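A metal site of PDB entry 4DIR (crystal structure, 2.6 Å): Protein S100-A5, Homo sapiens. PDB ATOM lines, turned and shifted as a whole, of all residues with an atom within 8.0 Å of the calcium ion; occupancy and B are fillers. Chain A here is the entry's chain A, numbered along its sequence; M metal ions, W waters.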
ATOM      1  N   PHE A  16      17.406 -23.131   1.528  1.00  0.00           N
ATOM      2  CA  PHE A  16      17.129 -21.844   0.901  1.00  0.00           C
ATOM      3  C   PHE A  16      15.861 -21.985   0.115  1.00  0.00           C
ATOM      4  O   PHE A  16      14.918 -21.214   0.316  1.00  0.00           O
ATOM      5  CB  PHE A  16      18.231 -21.448  -0.058  1.00  0.00           C
ATOM      6  CG  PHE A  16      17.942 -20.166  -0.804  1.00  0.00           C
ATOM      7  CD1 PHE A  16      18.173 -18.914  -0.196  1.00  0.00           C
ATOM      8  CD2 PHE A  16      17.464 -20.199  -2.113  1.00  0.00           C
ATOM      9  CE1 PHE A  16      17.953 -17.717  -0.868  1.00  0.00           C
ATOM     10  CE2 PHE A  16      17.221 -19.000  -2.828  1.00  0.00           C
ATOM     11  CZ  PHE A  16      17.473 -17.747  -2.210  1.00  0.00           C
ATOM     12  N   HIS A  17      15.842 -22.973  -0.787  1.00  0.00           N
ATOM     13  CA  HIS A  17      14.722 -23.176  -1.698  1.00  0.00           C
ATOM     14  C   HIS A  17      13.488 -23.701  -0.990  1.00  0.00           C
ATOM     15  O   HIS A  17      12.385 -23.448  -1.478  1.00  0.00           O
ATOM     16  CB  HIS A  17      15.126 -24.054  -2.897  1.00  0.00           C
ATOM     17  CG  HIS A  17      16.131 -23.389  -3.796  1.00  0.00           C
ATOM     18  ND1 HIS A  17      17.474 -23.681  -3.763  1.00  0.00           N
ATOM     19  CD2 HIS A  17      15.981 -22.421  -4.738  1.00  0.00           C
ATOM     20  CE1 HIS A  17      18.113 -22.948  -4.661  1.00  0.00           C
ATOM     21  NE2 HIS A  17      17.224 -22.164  -5.255  1.00  0.00           N
ATOM     22  N   TYR A  19      12.278 -22.372   1.298  1.00  0.00           N
ATOM     23  CA  TYR A  19      11.595 -21.157   1.762  1.00  0.00           C
ATOM     24  C   TYR A  19      11.457 -20.097   0.704  1.00  0.00           C
ATOM     25  O   TYR A  19      10.557 -19.272   0.772  1.00  0.00           O
ATOM     26  CB  TYR A  19      12.279 -20.575   3.002  1.00  0.00           C
ATOM     27  CG  TYR A  19      12.137 -21.458   4.234  1.00  0.00           C
ATOM     28  CD1 TYR A  19      13.057 -22.444   4.524  1.00  0.00           C
ATOM     29  CD2 TYR A  19      11.041 -21.326   5.072  1.00  0.00           C
ATOM     30  CE1 TYR A  19      12.908 -23.250   5.627  1.00  0.00           C
ATOM     31  CE2 TYR A  19      10.888 -22.146   6.164  1.00  0.00           C
ATOM     32  CZ  TYR A  19      11.813 -23.094   6.430  1.00  0.00           C
ATOM     33  OH  TYR A  19      11.616 -23.884   7.524  1.00  0.00           O
ATOM     34  N   SER A  20      12.346 -20.103  -0.291  1.00  0.00           N
ATOM     35  CA  SER A  20      12.322 -19.047  -1.318  1.00  0.00           C
ATOM     36  C   SER A  20      11.131 -19.093  -2.311  1.00  0.00           C
ATOM     37  O   SER A  20      10.680 -18.057  -2.799  1.00  0.00           O
ATOM     38  CB  SER A  20      13.630 -19.042  -2.104  1.00  0.00           C
ATOM     39  OG  SER A  20      13.825 -20.296  -2.730  1.00  0.00           O
ATOM     40  N   GLY A  21      10.657 -20.298  -2.609  1.00  0.00           N
ATOM     41  CA  GLY A  21       9.538 -20.473  -3.508  1.00  0.00           C
ATOM     42  C   GLY A  21       8.157 -20.379  -2.874  1.00  0.00           C
ATOM     43  O   GLY A  21       7.174 -20.646  -3.542  1.00  0.00           O
ATOM     44  N   ARG A  22       8.064 -19.909  -1.647  1.00  0.00           N
ATOM     45  CA  ARG A  22       6.757 -19.730  -1.060  1.00  0.00           C
ATOM     46  C   ARG A  22       6.014 -18.531  -1.605  1.00  0.00           C
ATOM     47  O   ARG A  22       4.818 -18.568  -1.748  1.00  0.00           O
ATOM     48  CB  ARG A  22       6.866 -19.640   0.444  1.00  0.00           C
ATOM     49  CG  ARG A  22       7.271 -20.932   1.004  1.00  0.00           C
ATOM     50  CD  ARG A  22       7.357 -20.900   2.473  1.00  0.00           C
ATOM     51  NE  ARG A  22       7.583 -22.244   2.967  1.00  0.00           N
ATOM     52  CZ  ARG A  22       7.555 -22.580   4.247  1.00  0.00           C
ATOM     53  NH1 ARG A  22       7.312 -21.675   5.159  1.00  0.00           N
ATOM     54  NH2 ARG A  22       7.788 -23.829   4.583  1.00  0.00           N
ATOM     55  N   GLU A  23       6.714 -17.468  -1.915  1.00  0.00           N
ATOM     56  CA  GLU A  23       6.053 -16.293  -2.480  1.00  0.00           C
ATOM     57  C   GLU A  23       7.023 -15.488  -3.323  1.00  0.00           C
ATOM     58  O   GLU A  23       8.223 -15.591  -3.141  1.00  0.00           O
ATOM     59  CB  GLU A  23       5.492 -15.427  -1.369  1.00  0.00           C
ATOM     60  CG  GLU A  23       6.556 -14.807  -0.473  1.00  0.00           C
ATOM     61  CD  GLU A  23       5.979 -14.043   0.711  1.00  0.00           C
ATOM     62  OE1 GLU A  23       5.331 -14.676   1.595  1.00  0.00           O
ATOM     63  OE2 GLU A  23       6.172 -12.803   0.728  1.00  0.00           O
ATOM     64  N   GLY A  24       6.501 -14.657  -4.221  1.00  0.00           N
ATOM     65  CA  GLY A  24       7.335 -13.870  -5.129  1.00  0.00           C
ATOM     66  C   GLY A  24       8.288 -14.780  -5.870  1.00  0.00           C
ATOM     67  O   GLY A  24       7.992 -15.972  -6.069  1.00  0.00           O
ATOM     68  N   SER A  25       9.452 -14.268  -6.249  1.00  0.00           N
ATOM     69  CA  SER A  25      10.361 -15.067  -7.008  1.00  0.00           C
ATOM     70  C   SER A  25      10.752 -16.319  -6.225  1.00  0.00           C
ATOM     71  O   SER A  25      10.873 -16.328  -5.013  1.00  0.00           O
ATOM     72  CB  SER A  25      11.591 -14.272  -7.412  1.00  0.00           C
ATOM     73  OG  SER A  25      12.638 -15.170  -7.796  1.00  0.00           O
ATOM     74  N   LYS A  26      10.936 -17.399  -6.954  1.00  0.00           N
ATOM     75  CA  LYS A  26      11.252 -18.651  -6.334  1.00  0.00           C
ATOM     76  C   LYS A  26      12.751 -18.703  -6.070  1.00  0.00           C
ATOM     77  O   LYS A  26      13.249 -19.611  -5.433  1.00  0.00           O
ATOM     78  CB  LYS A  26      10.825 -19.758  -7.286  1.00  0.00           C
ATOM     79  N   LEU A  27      13.442 -17.691  -6.602  1.00  0.00           N
ATOM     80  CA  LEU A  27      14.885 -17.536  -6.471  1.00  0.00           C
ATOM     81  C   LEU A  27      15.346 -16.546  -5.383  1.00  0.00           C
ATOM     82  O   LEU A  27      16.558 -16.324  -5.208  1.00  0.00           O
ATOM     83  CB  LEU A  27      15.425 -17.037  -7.811  1.00  0.00           C
ATOM     84  CG  LEU A  27      15.872 -17.967  -8.931  1.00  0.00           C
ATOM     85  CD1 LEU A  27      15.223 -19.329  -8.872  1.00  0.00           C
ATOM     86  CD2 LEU A  27      15.598 -17.266 -10.234  1.00  0.00           C
ATOM     87  N   THR A  28      14.406 -15.916  -4.680  1.00  0.00           N
ATOM     88  CA  THR A  28      14.786 -15.036  -3.598  1.00  0.00           C
ATOM     89  C   THR A  28      13.858 -15.198  -2.395  1.00  0.00           C
ATOM     90  O   THR A  28      12.722 -15.659  -2.505  1.00  0.00           O
ATOM     91  CB  THR A  28      14.743 -13.571  -3.992  1.00  0.00           C
ATOM     92  OG1 THR A  28      13.374 -13.228  -4.202  1.00  0.00           O
ATOM     93  CG2 THR A  28      15.642 -13.251  -5.231  1.00  0.00           C
ATOM     94  N   LEU A  29      14.394 -14.806  -1.241  1.00  0.00           N
ATOM     95  CA  LEU A  29      13.680 -14.826   0.035  1.00  0.00           C
ATOM     96  C   LEU A  29      13.183 -13.431   0.282  1.00  0.00           C
ATOM     97  O   LEU A  29      13.963 -12.504   0.299  1.00  0.00           O
ATOM     98  CB  LEU A  29      14.617 -15.213   1.170  1.00  0.00           C
ATOM     99  CG  LEU A  29      15.171 -16.624   1.231  1.00  0.00           C
ATOM    100  CD1 LEU A  29      16.395 -16.673   2.147  1.00  0.00           C
ATOM    101  CD2 LEU A  29      14.123 -17.535   1.807  1.00  0.00           C
ATOM    102  N   SER A  30      11.884 -13.283   0.470  1.00  0.00           N
ATOM    103  CA  SER A  30      11.330 -12.016   0.935  1.00  0.00           C
ATOM    104  C   SER A  30      11.651 -11.871   2.431  1.00  0.00           C
ATOM    105  O   SER A  30      12.217 -12.802   3.020  1.00  0.00           O
ATOM    106  CB  SER A  30       9.811 -11.992   0.702  1.00  0.00           C
ATOM    107  OG  SER A  30       9.119 -12.988   1.439  1.00  0.00           O
ATOM    108  N   ARG A  31      11.255 -10.777   3.034  1.00  0.00           N
ATOM    109  CA  ARG A  31      11.401 -10.611   4.464  1.00  0.00           C
ATOM    110  C   ARG A  31      10.644 -11.693   5.187  1.00  0.00           C
ATOM    111  O   ARG A  31      11.149 -12.284   6.101  1.00  0.00           O
ATOM    112  CB  ARG A  31      10.894  -9.241   4.885  1.00  0.00           C
ATOM    113  CG  ARG A  31      10.941  -9.001   6.381  1.00  0.00           C
ATOM    114  CD  ARG A  31      10.273  -7.692   6.782  1.00  0.00           C
ATOM    115  NE  ARG A  31      11.243  -6.648   7.019  1.00  0.00           N
ATOM    116  CZ  ARG A  31      11.796  -5.912   6.065  1.00  0.00           C
ATOM    117  NH1 ARG A  31      11.458  -6.097   4.802  1.00  0.00           N
ATOM    118  NH2 ARG A  31      12.675  -4.972   6.369  1.00  0.00           N
ATOM    119  N   GLU A  33       9.665 -14.768   4.101  1.00  0.00           N
ATOM    120  CA  GLU A  33      10.259 -16.091   3.895  1.00  0.00           C
ATOM    121  C   GLU A  33      11.505 -16.230   4.730  1.00  0.00           C
ATOM    122  O   GLU A  33      11.736 -17.294   5.297  1.00  0.00           O
ATOM    123  CB  GLU A  33      10.595 -16.305   2.415  1.00  0.00           C
ATOM    124  CG  GLU A  33       9.384 -16.226   1.504  1.00  0.00           C
ATOM    125  CD  GLU A  33       9.711 -16.352   0.053  1.00  0.00           C
ATOM    126  OE1 GLU A  33      10.644 -15.682  -0.470  1.00  0.00           O
ATOM    127  OE2 GLU A  33       9.006 -17.121  -0.607  1.00  0.00           O
ATOM    128  N   LEU A  34      12.281 -15.153   4.820  1.00  0.00           N
ATOM    129  CA  LEU A  34      13.481 -15.159   5.627  1.00  0.00           C
ATOM    130  C   LEU A  34      13.127 -15.435   7.045  1.00  0.00           C
ATOM    131  O   LEU A  34      13.746 -16.286   7.688  1.00  0.00           O
ATOM    132  CB  LEU A  34      14.147 -13.807   5.614  1.00  0.00           C
ATOM    133  CG  LEU A  34      15.684 -13.854   5.735  1.00  0.00           C
ATOM    134  CD1 LEU A  34      16.219 -12.523   6.287  1.00  0.00           C
ATOM    135  CD2 LEU A  34      16.299 -15.014   6.528  1.00  0.00           C
ATOM    136  N   GLU A  66      14.796  -8.262  -1.008  1.00  0.00           N
ATOM    137  CA  GLU A  66      14.723  -9.702  -1.173  1.00  0.00           C
ATOM    138  C   GLU A  66      16.094 -10.227  -0.992  1.00  0.00           C
ATOM    139  O   GLU A  66      17.051  -9.552  -1.325  1.00  0.00           O
ATOM    140  CB  GLU A  66      14.334 -10.086  -2.585  1.00  0.00           C
ATOM    141  CG  GLU A  66      13.087  -9.482  -3.122  1.00  0.00           C
ATOM    142  CD  GLU A  66      12.772 -10.031  -4.510  1.00  0.00           C
ATOM    143  OE1 GLU A  66      12.098 -11.055  -4.573  1.00  0.00           O
ATOM    144  OE2 GLU A  66      13.178  -9.457  -5.539  1.00  0.00           O
ATOM    145  N   ILE A  67      16.184 -11.417  -0.490  1.00  0.00           N
ATOM    146  CA  ILE A  67      17.470 -12.041  -0.290  1.00  0.00           C
ATOM    147  C   ILE A  67      17.732 -13.051  -1.418  1.00  0.00           C
ATOM    148  O   ILE A  67      17.109 -14.119  -1.476  1.00  0.00           O
ATOM    149  CB  ILE A  67      17.573 -12.640   1.139  1.00  0.00           C
ATOM    150  CG1 ILE A  67      17.328 -11.550   2.205  1.00  0.00           C
ATOM    151  CG2 ILE A  67      18.947 -13.263   1.372  1.00  0.00           C
ATOM    152  CD1 ILE A  67      18.311 -10.307   2.113  1.00  0.00           C
HETATM  153 CA    CA M   1      10.444 -15.864  -2.618  1.00  0.00          CA
HETATM  154  O   HOH W   1      10.881 -13.694  -3.230  1.00  0.00           O
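The side-chain carboxylate (OE1) of Glu 33 is bound to the calcium ion (2.2 Å).
O of Ser 20 is bound to the calcium ion (2.2 Å).
O of Thr 28 binds the calcium ion, at 2.3 Å.
The calcium ion is bound by water W1 (2.3 Å).
The calcium ion is bound by O of Glu 23 (2.3 Å).
O of Ser 25 is bound to the calcium ion, 2.5 Å away.
The calcium ion is bound by the side-chain carboxylate (OE2) of Glu 33 (2.8 Å).
The side-chain hydroxyl of Ser 20 sits at hydrogen-bond distance from the backbone carbonyl oxygen of Phe 16, 3.4 Å away.
The backbone carbonyl oxygen (O) of Lys 26 lies within hydrogen-bond range of the side-chain hydroxyl (OG) of Ser 20.
The backbone NH (N) of Leu 27 is in hydrogen-bond range of the side-chain hydroxyl (OG) of Ser 25 (2.9 Å).
The backbone NH (N) of Arg 22 sits close to the side-chain carboxylate (OE2) of Glu 33, at 3.1 Å.
N of Glu 33 sits at hydrogen-bond distance from OG of Ser 30, at 3.2 Å.
OG of Ser 30 lies within hydrogen-bond range of OE2 of Glu 23 (3.0 Å).
The side-chain hydroxyl of Thr 28 lies within hydrogen-bond range of the side-chain carboxylate of Glu 66 (2.5 Å).
Water W1 lies within hydrogen-bond range of the side-chain hydroxyl (OG1) of Thr 28, the side-chain carboxylate (OE1) of Glu 66 and the backbone NH (N) of Ser 25.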
